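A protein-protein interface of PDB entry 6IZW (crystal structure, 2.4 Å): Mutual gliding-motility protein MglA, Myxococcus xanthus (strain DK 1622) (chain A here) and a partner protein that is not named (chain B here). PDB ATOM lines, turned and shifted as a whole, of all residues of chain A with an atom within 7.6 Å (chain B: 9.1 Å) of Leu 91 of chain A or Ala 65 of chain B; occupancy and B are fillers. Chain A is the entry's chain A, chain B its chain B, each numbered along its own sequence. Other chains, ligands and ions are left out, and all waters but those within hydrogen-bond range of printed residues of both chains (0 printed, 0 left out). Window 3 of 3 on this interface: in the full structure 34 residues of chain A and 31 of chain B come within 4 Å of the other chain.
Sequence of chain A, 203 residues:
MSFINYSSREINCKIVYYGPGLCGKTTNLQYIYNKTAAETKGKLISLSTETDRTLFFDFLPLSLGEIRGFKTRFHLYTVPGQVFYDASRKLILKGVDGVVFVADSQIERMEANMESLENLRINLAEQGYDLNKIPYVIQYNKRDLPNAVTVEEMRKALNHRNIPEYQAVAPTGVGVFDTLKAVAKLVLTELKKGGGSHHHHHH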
ATOM      1  N   LYS A  14     -36.910 -18.488  -1.102  1.00  0.00           N
ATOM      2  CA  LYS A  14     -36.411 -18.896  -2.407  1.00  0.00           C
ATOM      3  C   LYS A  14     -36.366 -20.419  -2.473  1.00  0.00           C
ATOM      4  O   LYS A  14     -35.708 -21.069  -1.650  1.00  0.00           O
ATOM      5  CB  LYS A  14     -35.030 -18.291  -2.673  1.00  0.00           C
ATOM      6  CG  LYS A  14     -34.462 -18.700  -4.038  1.00  0.00           C
ATOM      7  CD  LYS A  14     -33.348 -17.768  -4.472  1.00  0.00           C
ATOM      8  CE  LYS A  14     -32.488 -18.394  -5.529  1.00  0.00           C
ATOM      9  NZ  LYS A  14     -31.504 -17.379  -5.999  1.00  0.00           N
ATOM     10  N   VAL A  16     -35.592 -23.695  -5.101  1.00  0.00           N
ATOM     11  CA  VAL A  16     -34.925 -24.043  -6.341  1.00  0.00           C
ATOM     12  C   VAL A  16     -35.248 -25.488  -6.672  1.00  0.00           C
ATOM     13  O   VAL A  16     -35.096 -26.377  -5.822  1.00  0.00           O
ATOM     14  CB  VAL A  16     -33.405 -23.818  -6.257  1.00  0.00           C
ATOM     15  CG1 VAL A  16     -32.748 -24.408  -7.479  1.00  0.00           C
ATOM     16  CG2 VAL A  16     -33.119 -22.316  -6.154  1.00  0.00           C
ATOM     17  N   PHE A  56     -30.934 -20.862 -18.545  1.00  0.00           N
ATOM     18  CA  PHE A  56     -30.380 -20.202 -17.375  1.00  0.00           C
ATOM     19  C   PHE A  56     -31.253 -20.494 -16.167  1.00  0.00           C
ATOM     20  O   PHE A  56     -30.785 -21.103 -15.211  1.00  0.00           O
ATOM     21  CB  PHE A  56     -30.253 -18.700 -17.625  1.00  0.00           C
ATOM     22  CG  PHE A  56     -29.359 -17.982 -16.643  1.00  0.00           C
ATOM     23  CD1 PHE A  56     -28.677 -18.674 -15.660  1.00  0.00           C
ATOM     24  CD2 PHE A  56     -29.208 -16.601 -16.723  1.00  0.00           C
ATOM     25  CE1 PHE A  56     -27.868 -18.009 -14.754  1.00  0.00           C
ATOM     26  CE2 PHE A  56     -28.400 -15.919 -15.823  1.00  0.00           C
ATOM     27  CZ  PHE A  56     -27.721 -16.628 -14.830  1.00  0.00           C
ATOM     28  N   PHE A  57     -32.500 -20.032 -16.166  1.00  0.00           N
ATOM     29  CA  PHE A  57     -33.452 -20.423 -15.133  1.00  0.00           C
ATOM     30  C   PHE A  57     -34.855 -20.170 -15.653  1.00  0.00           C
ATOM     31  O   PHE A  57     -35.039 -19.448 -16.637  1.00  0.00           O
ATOM     32  CB  PHE A  57     -33.230 -19.661 -13.817  1.00  0.00           C
ATOM     33  CG  PHE A  57     -33.278 -18.169 -13.967  1.00  0.00           C
ATOM     34  CD1 PHE A  57     -34.492 -17.476 -13.857  1.00  0.00           C
ATOM     35  CD2 PHE A  57     -32.107 -17.445 -14.235  1.00  0.00           C
ATOM     36  CE1 PHE A  57     -34.538 -16.081 -13.986  1.00  0.00           C
ATOM     37  CE2 PHE A  57     -32.134 -16.065 -14.370  1.00  0.00           C
ATOM     38  CZ  PHE A  57     -33.355 -15.370 -14.233  1.00  0.00           C
ATOM     39  N   VAL A  79     -33.353 -24.805 -12.350  1.00  0.00           N
ATOM     40  CA  VAL A  79     -32.015 -24.669 -12.908  1.00  0.00           C
ATOM     41  C   VAL A  79     -32.006 -25.294 -14.301  1.00  0.00           C
ATOM     42  O   VAL A  79     -32.915 -26.064 -14.634  1.00  0.00           O
ATOM     43  CB  VAL A  79     -30.969 -25.344 -11.998  1.00  0.00           C
ATOM     44  CG1 VAL A  79     -31.029 -24.766 -10.599  1.00  0.00           C
ATOM     45  CG2 VAL A  79     -31.183 -26.874 -11.979  1.00  0.00           C
ATOM     46  N   TYR A  85     -24.265 -27.001 -18.299  1.00  0.00           N
ATOM     47  CA  TYR A  85     -24.691 -25.700 -17.791  1.00  0.00           C
ATOM     48  C   TYR A  85     -24.308 -25.494 -16.334  1.00  0.00           C
ATOM     49  O   TYR A  85     -24.813 -24.562 -15.697  1.00  0.00           O
ATOM     50  CB  TYR A  85     -26.204 -25.528 -17.932  1.00  0.00           C
ATOM     51  CG  TYR A  85     -26.733 -25.432 -19.349  1.00  0.00           C
ATOM     52  CD1 TYR A  85     -26.279 -24.454 -20.221  1.00  0.00           C
ATOM     53  CD2 TYR A  85     -27.728 -26.295 -19.795  1.00  0.00           C
ATOM     54  CE1 TYR A  85     -26.786 -24.364 -21.522  1.00  0.00           C
ATOM     55  CE2 TYR A  85     -28.248 -26.209 -21.070  1.00  0.00           C
ATOM     56  CZ  TYR A  85     -27.771 -25.247 -21.935  1.00  0.00           C
ATOM     57  OH  TYR A  85     -28.287 -25.170 -23.208  1.00  0.00           O
ATOM     58  N   ASP A  86     -23.463 -26.367 -15.786  1.00  0.00           N
ATOM     59  CA  ASP A  86     -23.092 -26.326 -14.374  1.00  0.00           C
ATOM     60  C   ASP A  86     -22.768 -24.924 -13.864  1.00  0.00           C
ATOM     61  O   ASP A  86     -23.204 -24.535 -12.774  1.00  0.00           O
ATOM     62  CB  ASP A  86     -21.900 -27.259 -14.138  1.00  0.00           C
ATOM     63  CG  ASP A  86     -21.714 -27.605 -12.656  1.00  0.00           C
ATOM     64  OD1 ASP A  86     -22.677 -28.100 -12.009  1.00  0.00           O
ATOM     65  OD2 ASP A  86     -20.598 -27.387 -12.132  1.00  0.00           O
ATOM     66  N   ALA A  87     -21.991 -24.153 -14.632  1.00  0.00           N
ATOM     67  CA  ALA A  87     -21.607 -22.816 -14.183  1.00  0.00           C
ATOM     68  C   ALA A  87     -22.824 -21.922 -13.974  1.00  0.00           C
ATOM     69  O   ALA A  87     -22.883 -21.174 -12.998  1.00  0.00           O
ATOM     70  CB  ALA A  87     -20.645 -22.179 -15.186  1.00  0.00           C
ATOM     71  N   SER A  88     -23.787 -21.955 -14.901  1.00  0.00           N
ATOM     72  CA  SER A  88     -25.032 -21.213 -14.708  1.00  0.00           C
ATOM     73  C   SER A  88     -25.871 -21.825 -13.585  1.00  0.00           C
ATOM     74  O   SER A  88     -26.523 -21.110 -12.814  1.00  0.00           O
ATOM     75  CB  SER A  88     -25.829 -21.187 -16.017  1.00  0.00           C
ATOM     76  OG  SER A  88     -25.119 -20.574 -17.099  1.00  0.00           O
ATOM     77  N   ARG A  89     -25.859 -23.147 -13.481  1.00  0.00           N
ATOM     78  CA  ARG A  89     -26.652 -23.835 -12.469  1.00  0.00           C
ATOM     79  C   ARG A  89     -26.209 -23.436 -11.060  1.00  0.00           C
ATOM     80  O   ARG A  89     -27.054 -23.212 -10.177  1.00  0.00           O
ATOM     81  CB  ARG A  89     -26.555 -25.350 -12.716  1.00  0.00           C
ATOM     82  CG  ARG A  89     -27.218 -26.251 -11.728  1.00  0.00           C
ATOM     83  CD  ARG A  89     -27.471 -27.649 -12.317  1.00  0.00           C
ATOM     84  NE  ARG A  89     -26.238 -28.370 -12.631  1.00  0.00           N
ATOM     85  CZ  ARG A  89     -25.789 -28.657 -13.859  1.00  0.00           C
ATOM     86  NH1 ARG A  89     -26.455 -28.305 -14.942  1.00  0.00           N
ATOM     87  NH2 ARG A  89     -24.649 -29.300 -14.009  1.00  0.00           N
ATOM     88  N   LYS A  90     -24.894 -23.279 -10.836  1.00  0.00           N
ATOM     89  CA  LYS A  90     -24.433 -22.871  -9.501  1.00  0.00           C
ATOM     90  C   LYS A  90     -24.977 -21.509  -9.100  1.00  0.00           C
ATOM     91  O   LYS A  90     -25.182 -21.247  -7.910  1.00  0.00           O
ATOM     92  CB  LYS A  90     -22.909 -22.789  -9.424  1.00  0.00           C
ATOM     93  CG  LYS A  90     -22.156 -24.053  -9.679  1.00  0.00           C
ATOM     94  CD  LYS A  90     -20.675 -23.707  -9.787  1.00  0.00           C
ATOM     95  CE  LYS A  90     -19.825 -24.956  -9.919  1.00  0.00           C
ATOM     96  NZ  LYS A  90     -18.722 -24.980  -8.914  1.00  0.00           N
ATOM     97  N   LEU A  91     -25.150 -20.607 -10.061  1.00  0.00           N
ATOM     98  CA  LEU A  91     -25.577 -19.257  -9.711  1.00  0.00           C
ATOM     99  C   LEU A  91     -26.945 -19.255  -9.042  1.00  0.00           C
ATOM    100  O   LEU A  91     -27.221 -18.393  -8.196  1.00  0.00           O
ATOM    101  CB  LEU A  91     -25.606 -18.390 -10.963  1.00  0.00           C
ATOM    102  CG  LEU A  91     -24.330 -18.373 -11.805  1.00  0.00           C
ATOM    103  CD1 LEU A  91     -24.537 -17.442 -12.987  1.00  0.00           C
ATOM    104  CD2 LEU A  91     -23.148 -17.912 -10.951  1.00  0.00           C
ATOM    105  N   ILE A  92     -27.819 -20.196  -9.422  1.00  0.00           N
ATOM    106  CA  ILE A  92     -29.210 -20.145  -8.989  1.00  0.00           C
ATOM    107  C   ILE A  92     -29.331 -20.522  -7.519  1.00  0.00           C
ATOM    108  O   ILE A  92     -30.267 -20.092  -6.840  1.00  0.00           O
ATOM    109  CB  ILE A  92     -30.086 -21.049  -9.886  1.00  0.00           C
ATOM    110  CG1 ILE A  92     -29.787 -20.801 -11.368  1.00  0.00           C
ATOM    111  CG2 ILE A  92     -31.551 -20.785  -9.625  1.00  0.00           C
ATOM    112  CD1 ILE A  92     -29.995 -19.344 -11.749  1.00  0.00           C
ATOM    113  N   LEU A  93     -28.385 -21.300  -6.997  1.00  0.00           N
ATOM    114  CA  LEU A  93     -28.444 -21.747  -5.614  1.00  0.00           C
ATOM    115  C   LEU A  93     -28.135 -20.644  -4.604  1.00  0.00           C
ATOM    116  O   LEU A  93     -28.278 -20.878  -3.394  1.00  0.00           O
ATOM    117  CB  LEU A  93     -27.481 -22.919  -5.411  1.00  0.00           C
ATOM    118  CG  LEU A  93     -27.844 -24.240  -6.093  1.00  0.00           C
ATOM    119  CD1 LEU A  93     -26.782 -25.246  -5.784  1.00  0.00           C
ATOM    120  CD2 LEU A  93     -29.185 -24.774  -5.634  1.00  0.00           C
ATOM    121  N   LYS A  94     -27.744 -19.450  -5.041  1.00  0.00           N
ATOM    122  CA  LYS A  94     -27.344 -18.437  -4.070  1.00  0.00           C
ATOM    123  C   LYS A  94     -28.549 -18.013  -3.240  1.00  0.00           C
ATOM    124  O   LYS A  94     -29.590 -17.622  -3.783  1.00  0.00           O
ATOM    125  CB  LYS A  94     -26.695 -17.232  -4.765  1.00  0.00           C
ATOM    126  CG  LYS A  94     -26.625 -15.942  -3.926  1.00  0.00           C
ATOM    127  CD  LYS A  94     -26.026 -16.209  -2.510  1.00  0.00           C
ATOM    128  CE  LYS A  94     -24.555 -15.854  -2.270  1.00  0.00           C
ATOM    129  NZ  LYS A  94     -24.520 -15.400  -0.816  1.00  0.00           N
ATOM    130  N   GLY A  95     -28.398 -18.093  -1.921  1.00  0.00           N
ATOM    131  CA  GLY A  95     -29.462 -17.721  -1.016  1.00  0.00           C
ATOM    132  C   GLY A  95     -30.667 -18.642  -1.007  1.00  0.00           C
ATOM    133  O   GLY A  95     -31.754 -18.214  -0.625  1.00  0.00           O
ATOM    134  N   ASN A 123     -22.391 -28.545  -5.220  1.00  0.00           N
ATOM    135  CA  ASN A 123     -22.590 -27.117  -5.449  1.00  0.00           C
ATOM    136  C   ASN A 123     -23.002 -26.405  -4.170  1.00  0.00           C
ATOM    137  O   ASN A 123     -22.590 -25.267  -3.926  1.00  0.00           O
ATOM    138  CB  ASN A 123     -23.622 -26.895  -6.559  1.00  0.00           C
ATOM    139  CG  ASN A 123     -23.021 -27.111  -7.941  1.00  0.00           C
ATOM    140  OD1 ASN A 123     -21.806 -27.181  -8.079  1.00  0.00           O
ATOM    141  ND2 ASN A 123     -23.858 -27.228  -8.955  1.00  0.00           N
ATOM    142  N   GLN A 127     -20.607 -23.377  -1.792  1.00  0.00           N
ATOM    143  CA  GLN A 127     -20.997 -22.038  -1.372  1.00  0.00           C
ATOM    144  C   GLN A 127     -21.412 -21.996   0.091  1.00  0.00           C
ATOM    145  O   GLN A 127     -22.039 -21.029   0.531  1.00  0.00           O
ATOM    146  CB  GLN A 127     -22.104 -21.493  -2.268  1.00  0.00           C
ATOM    147  CG  GLN A 127     -23.371 -22.273  -2.184  1.00  0.00           C
ATOM    148  CD  GLN A 127     -24.419 -21.679  -3.079  1.00  0.00           C
ATOM    149  OE1 GLN A 127     -24.167 -21.410  -4.273  1.00  0.00           O
ATOM    150  NE2 GLN A 127     -25.604 -21.445  -2.515  1.00  0.00           N
ATOM    151  N   LYS B  36     -28.386  -9.580  -4.634  1.00  0.00           N
ATOM    152  CA  LYS B  36     -27.743 -10.447  -5.608  1.00  0.00           C
ATOM    153  C   LYS B  36     -28.508 -11.757  -5.789  1.00  0.00           C
ATOM    154  O   LYS B  36     -28.550 -12.305  -6.900  1.00  0.00           O
ATOM    155  CB  LYS B  36     -26.297 -10.715  -5.190  1.00  0.00           C
ATOM    156  CG  LYS B  36     -25.302  -9.719  -5.791  1.00  0.00           C
ATOM    157  CD  LYS B  36     -23.868 -10.091  -5.452  1.00  0.00           C
ATOM    158  CE  LYS B  36     -22.926  -8.929  -5.777  1.00  0.00           C
ATOM    159  NZ  LYS B  36     -21.503  -9.315  -5.614  1.00  0.00           N
ATOM    160  N   ASN B  37     -29.138 -12.261  -4.730  1.00  0.00           N
ATOM    161  CA  ASN B  37     -29.828 -13.536  -4.829  1.00  0.00           C
ATOM    162  C   ASN B  37     -31.154 -13.421  -5.560  1.00  0.00           C
ATOM    163  O   ASN B  37     -31.828 -14.439  -5.725  1.00  0.00           O
ATOM    164  CB  ASN B  37     -30.036 -14.149  -3.435  1.00  0.00           C
ATOM    165  CG  ASN B  37     -30.928 -13.296  -2.517  1.00  0.00           C
ATOM    166  OD1 ASN B  37     -31.840 -12.583  -2.962  1.00  0.00           O
ATOM    167  ND2 ASN B  37     -30.667 -13.386  -1.221  1.00  0.00           N
ATOM    168  N   GLY B  38     -31.542 -12.217  -5.984  1.00  0.00           N
ATOM    169  CA  GLY B  38     -32.760 -11.991  -6.737  1.00  0.00           C
ATOM    170  C   GLY B  38     -33.830 -11.221  -5.992  1.00  0.00           C
ATOM    171  O   GLY B  38     -34.816 -10.807  -6.618  1.00  0.00           O
ATOM    172  N   SER B  57     -35.380 -10.119 -10.921  1.00  0.00           N
ATOM    173  CA  SER B  57     -34.890 -11.488 -11.055  1.00  0.00           C
ATOM    174  C   SER B  57     -33.932 -11.615 -12.237  1.00  0.00           C
ATOM    175  O   SER B  57     -32.902 -12.286 -12.141  1.00  0.00           O
ATOM    176  CB  SER B  57     -36.077 -12.447 -11.209  1.00  0.00           C
ATOM    177  OG  SER B  57     -35.649 -13.791 -11.241  1.00  0.00           O
ATOM    178  N   LEU B  58     -34.275 -10.978 -13.356  1.00  0.00           N
ATOM    179  CA  LEU B  58     -33.387 -10.935 -14.506  1.00  0.00           C
ATOM    180  C   LEU B  58     -32.126 -10.139 -14.191  1.00  0.00           C
ATOM    181  O   LEU B  58     -31.021 -10.516 -14.604  1.00  0.00           O
ATOM    182  CB  LEU B  58     -34.127 -10.326 -15.690  1.00  0.00           C
ATOM    183  CG  LEU B  58     -35.340 -11.104 -16.177  1.00  0.00           C
ATOM    184  CD1 LEU B  58     -36.238 -10.191 -16.999  1.00  0.00           C
ATOM    185  CD2 LEU B  58     -34.894 -12.320 -17.001  1.00  0.00           C
ATOM    186  N   THR B  59     -32.276  -9.048 -13.439  1.00  0.00           N
ATOM    187  CA  THR B  59     -31.126  -8.234 -13.087  1.00  0.00           C
ATOM    188  C   THR B  59     -30.125  -9.048 -12.295  1.00  0.00           C
ATOM    189  O   THR B  59     -28.936  -9.085 -12.629  1.00  0.00           O
ATOM    190  CB  THR B  59     -31.577  -7.001 -12.302  1.00  0.00           C
ATOM    191  OG1 THR B  59     -32.260  -6.101 -13.187  1.00  0.00           O
ATOM    192  CG2 THR B  59     -30.386  -6.291 -11.669  1.00  0.00           C
ATOM    193  N   ALA B  60     -30.586  -9.730 -11.247  1.00  0.00           N
ATOM    194  CA  ALA B  60     -29.648 -10.477 -10.422  1.00  0.00           C
ATOM    195  C   ALA B  60     -29.072 -11.657 -11.180  1.00  0.00           C
ATOM    196  O   ALA B  60     -27.936 -12.070 -10.914  1.00  0.00           O
ATOM    197  CB  ALA B  60     -30.322 -10.940  -9.133  1.00  0.00           C
ATOM    198  N   GLY B  61     -29.837 -12.221 -12.119  1.00  0.00           N
ATOM    199  CA  GLY B  61     -29.288 -13.255 -12.979  1.00  0.00           C
ATOM    200  C   GLY B  61     -28.207 -12.709 -13.894  1.00  0.00           C
ATOM    201  O   GLY B  61     -27.122 -13.288 -14.014  1.00  0.00           O
ATOM    202  N   ASN B  62     -28.486 -11.576 -14.538  1.00  0.00           N
ATOM    203  CA  ASN B  62     -27.486 -10.922 -15.374  1.00  0.00           C
ATOM    204  C   ASN B  62     -26.211 -10.633 -14.582  1.00  0.00           C
ATOM    205  O   ASN B  62     -25.114 -11.048 -14.980  1.00  0.00           O
ATOM    206  CB  ASN B  62     -28.076  -9.640 -15.965  1.00  0.00           C
ATOM    207  CG  ASN B  62     -27.039  -8.764 -16.637  1.00  0.00           C
ATOM    208  OD1 ASN B  62     -25.949  -9.211 -16.974  1.00  0.00           O
ATOM    209  ND2 ASN B  62     -27.374  -7.501 -16.829  1.00  0.00           N
ATOM    210  N   VAL B  63     -26.340  -9.952 -13.441  1.00  0.00           N
ATOM    211  CA  VAL B  63     -25.163  -9.564 -12.665  1.00  0.00           C
ATOM    212  C   VAL B  63     -24.390 -10.792 -12.213  1.00  0.00           C
ATOM    213  O   VAL B  63     -23.154 -10.799 -12.230  1.00  0.00           O
ATOM    214  CB  VAL B  63     -25.571  -8.681 -11.467  1.00  0.00           C
ATOM    215  CG1 VAL B  63     -24.465  -8.666 -10.396  1.00  0.00           C
ATOM    216  CG2 VAL B  63     -25.909  -7.272 -11.942  1.00  0.00           C
ATOM    217  N   ALA B  64     -25.099 -11.857 -11.818  1.00  0.00           N
ATOM    218  CA  ALA B  64     -24.411 -13.074 -11.393  1.00  0.00           C
ATOM    219  C   ALA B  64     -23.668 -13.735 -12.552  1.00  0.00           C
ATOM    220  O   ALA B  64     -22.599 -14.331 -12.350  1.00  0.00           O
ATOM    221  CB  ALA B  64     -25.404 -14.052 -10.768  1.00  0.00           C
ATOM    222  N   ALA B  65     -24.230 -13.677 -13.767  1.00  0.00           N
ATOM    223  CA  ALA B  65     -23.530 -14.259 -14.909  1.00  0.00           C
ATOM    224  C   ALA B  65     -22.291 -13.441 -15.258  1.00  0.00           C
ATOM    225  O   ALA B  65     -21.234 -14.004 -15.561  1.00  0.00           O
ATOM    226  CB  ALA B  65     -24.464 -14.376 -16.118  1.00  0.00           C
ATOM    227  N   MET B  66     -22.397 -12.120 -15.202  1.00  0.00           N
ATOM    228  CA  MET B  66     -21.233 -11.260 -15.388  1.00  0.00           C
ATOM    229  C   MET B  66     -20.222 -11.485 -14.290  1.00  0.00           C
ATOM    230  O   MET B  66     -19.019 -11.446 -14.543  1.00  0.00           O
ATOM    231  CB  MET B  66     -21.626  -9.789 -15.426  1.00  0.00           C
ATOM    232  CG  MET B  66     -22.233  -9.372 -16.753  1.00  0.00           C
ATOM    233  SD  MET B  66     -21.222 -10.044 -18.303  1.00  0.00           S
ATOM    234  CE  MET B  66     -19.460  -9.347 -17.837  1.00  0.00           C
ATOM    235  N   GLY B  67     -20.724 -11.735 -13.076  1.00  0.00           N
ATOM    236  CA  GLY B  67     -19.836 -12.063 -11.974  1.00  0.00           C
ATOM    237  C   GLY B  67     -18.947 -13.248 -12.287  1.00  0.00           C
ATOM    238  O   GLY B  67     -17.724 -13.178 -12.142  1.00  0.00           O
ATOM    239  N   GLY B  68     -19.548 -14.347 -12.752  1.00  0.00           N
ATOM    240  CA  GLY B  68     -18.765 -15.527 -13.081  1.00  0.00           C
ATOM    241  C   GLY B  68     -17.823 -15.319 -14.255  1.00  0.00           C
ATOM    242  O   GLY B  68     -16.742 -15.910 -14.294  1.00  0.00           O
ATOM    243  N   LEU B  69     -18.221 -14.486 -15.227  1.00  0.00           N
ATOM    244  CA  LEU B  69     -17.371 -14.220 -16.387  1.00  0.00           C
ATOM    245  C   LEU B  69     -16.162 -13.381 -15.997  1.00  0.00           C
ATOM    246  O   LEU B  69     -15.026 -13.712 -16.353  1.00  0.00           O
ATOM    247  CB  LEU B  69     -18.166 -13.514 -17.482  1.00  0.00           C
ATOM    248  CG  LEU B  69     -19.155 -14.361 -18.276  1.00  0.00           C
ATOM    249  CD1 LEU B  69     -20.174 -13.464 -18.989  1.00  0.00           C
ATOM    250  CD2 LEU B  69     -18.446 -15.282 -19.256  1.00  0.00           C
ATOM    251  N   ALA B  70     -16.395 -12.280 -15.273  1.00  0.00           N
ATOM    252  CA  ALA B  70     -15.295 -11.509 -14.703  1.00  0.00           C
ATOM    253  C   ALA B  70     -14.309 -12.419 -13.974  1.00  0.00           C
ATOM    254  O   ALA B  70     -13.100 -12.359 -14.214  1.00  0.00           O
ATOM    255  CB  ALA B  70     -15.840 -10.430 -13.768  1.00  0.00           C
ATOM    256  N   LYS B  71     -14.817 -13.307 -13.115  1.00  0.00           N
ATOM    257  CA  LYS B  71     -13.945 -14.246 -12.413  1.00  0.00           C
ATOM    258  C   LYS B  71     -13.213 -15.187 -13.368  1.00  0.00           C
ATOM    259  O   LYS B  71     -12.120 -15.668 -13.044  1.00  0.00           O
ATOM    260  CB  LYS B  71     -14.757 -15.053 -11.413  1.00  0.00           C
ATOM    261  CG  LYS B  71     -14.062 -15.338 -10.103  1.00  0.00           C
ATOM    262  CD  LYS B  71     -15.084 -15.705  -9.013  1.00  0.00           C
ATOM    263  CE  LYS B  71     -15.942 -14.499  -8.609  1.00  0.00           C
ATOM    264  NZ  LYS B  71     -16.962 -14.848  -7.568  1.00  0.00           N
ATOM    265  N   LEU B  72     -13.790 -15.469 -14.537  1.00  0.00           N
ATOM    266  CA  LEU B  72     -13.184 -16.443 -15.444  1.00  0.00           C
ATOM    267  C   LEU B  72     -11.974 -15.852 -16.164  1.00  0.00           C
ATOM    268  O   LEU B  72     -10.986 -16.553 -16.406  1.00  0.00           O
ATOM    269  CB  LEU B  72     -14.234 -16.938 -16.443  1.00  0.00           C
ATOM    270  CG  LEU B  72     -14.310 -18.410 -16.868  1.00  0.00           C
ATOM    271  CD1 LEU B  72     -13.876 -19.374 -15.765  1.00  0.00           C
ATOM    272  CD2 LEU B  72     -15.728 -18.735 -17.324  1.00  0.00           C
ATOM    273  N   GLU B  77     -15.613  -8.381  -9.869  1.00  0.00           N
ATOM    274  CA  GLU B  77     -16.948  -8.086 -10.378  1.00  0.00           C
ATOM    275  C   GLU B  77     -16.966  -6.689 -10.980  1.00  0.00           C
ATOM    276  O   GLU B  77     -16.554  -5.719 -10.335  1.00  0.00           O
ATOM    277  CB  GLU B  77     -17.986  -8.216  -9.255  1.00  0.00           C
ATOM    278  CG  GLU B  77     -19.455  -8.307  -9.722  1.00  0.00           C
ATOM    279  CD  GLU B  77     -20.266  -9.418  -9.012  1.00  0.00           C
ATOM    280  OE1 GLU B  77     -19.756 -10.029  -8.040  1.00  0.00           O
ATOM    281  OE2 GLU B  77     -21.423  -9.677  -9.427  1.00  0.00           O
ATOM    282  N   PHE B  78     -17.382  -6.594 -12.236  1.00  0.00           N
ATOM    283  CA  PHE B  78     -17.437  -5.299 -12.893  1.00  0.00           C
ATOM    284  C   PHE B  78     -18.324  -4.370 -12.079  1.00  0.00           C
ATOM    285  O   PHE B  78     -19.513  -4.668 -11.895  1.00  0.00           O
ATOM    286  CB  PHE B  78     -17.954  -5.427 -14.324  1.00  0.00           C
ATOM    287  CG  PHE B  78     -17.077  -6.274 -15.201  1.00  0.00           C
ATOM    288  CD1 PHE B  78     -15.878  -5.783 -15.688  1.00  0.00           C
ATOM    289  CD2 PHE B  78     -17.436  -7.571 -15.521  1.00  0.00           C
ATOM    290  CE1 PHE B  78     -15.059  -6.561 -16.495  1.00  0.00           C
ATOM    291  CE2 PHE B  78     -16.620  -8.352 -16.325  1.00  0.00           C
ATOM    292  CZ  PHE B  78     -15.432  -7.843 -16.813  1.00  0.00           C
ATOM    293  N   GLN B  81     -22.561  -1.706 -15.071  1.00  0.00           N
ATOM    294  CA  GLN B  81     -22.848  -2.148 -16.427  1.00  0.00           C
ATOM    295  C   GLN B  81     -23.702  -1.070 -17.068  1.00  0.00           C
ATOM    296  O   GLN B  81     -24.520  -0.430 -16.398  1.00  0.00           O
ATOM    297  CB  GLN B  81     -23.598  -3.488 -16.472  1.00  0.00           C
ATOM    298  CG  GLN B  81     -23.083  -4.564 -15.516  1.00  0.00           C
ATOM    299  CD  GLN B  81     -23.586  -5.960 -15.857  1.00  0.00           C
ATOM    300  OE1 GLN B  81     -24.351  -6.144 -16.811  1.00  0.00           O
ATOM    301  NE2 GLN B  81     -23.232  -6.935 -15.019  1.00  0.00           N
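The side-chain amino group (NZ) of Lys 14 of chain A sits at hydrogen-bond distance from the backbone carbonyl oxygen (O) of Asn 37 of chain B (3.0 Å).
Gly 61 of chain B touches Phe 56 of chain A (O to CE2, 3.4 Å). Ser 57 of chain B touches Phe 57 of chain A (OG to CE1, 3.7 Å). Leu 91 of chain A touches Ala 64 of chain B. Leu 91 of chain A touches Ala 65 of chain B. O of Lys 94 of chain A touches CB of Asn 37 of chain B, 3.5 Å away.
Leu 91 of chain A touches just these residues of chain B: Ala 64 (3.7 Å) and Ala 65 (3.9 Å). Of the printed residues of chain A, Ala 65 of chain B touches Leu 91 (3.9 Å). No residue of chain B comes within 4 Å of Ile 92 of chain A. Printed residues of chain A within 4 Å of Ala 64 of chain B: Leu 91 (3.7 Å). Printed residues of chain B within 4 Å of Lys 14 of chain A: Asn 37. Of the printed residues of chain B, Lys 94 of chain A touches Asn 37 (3.5 Å). Of the printed residues of chain A, Gly 61 of chain B touches Phe 56. The nearest residue of chain B that does not touch Leu 91 of chain A is Gly 61 of chain B (5.0 Å). The nearest printed residue of chain B that does not touch Lys 94 of chain A is Lys 36 of chain B (5.0 Å).
The side-chain amino group of Lys 14 of chain A sits close to the backbone carbonyl oxygen of Ile 92 of chain A. The backbone carbonyl oxygen of Lys 94 of chain A lies within hydrogen-bond range of the side-chain amino group of Lys 14 of chain A, at 2.9 Å.
Printed residues of chain A that touch a printed residue of chain B: Lys 14, Phe 56, Phe 57, Leu 91 and Lys 94. Hydrophobic or aromatic side chains of chain A that line the printed part of chain B: Phe 56, Phe 57 and Leu 91. Of the 22 printed residues of chain B, 5 touch a printed residue of chain A. Among the printed residues, 6 pairs touch across the chains. Among the printed residues, no Asp or Glu carboxylate lies within 4 Å of a Lys or Arg side-chain nitrogen of the other chain.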
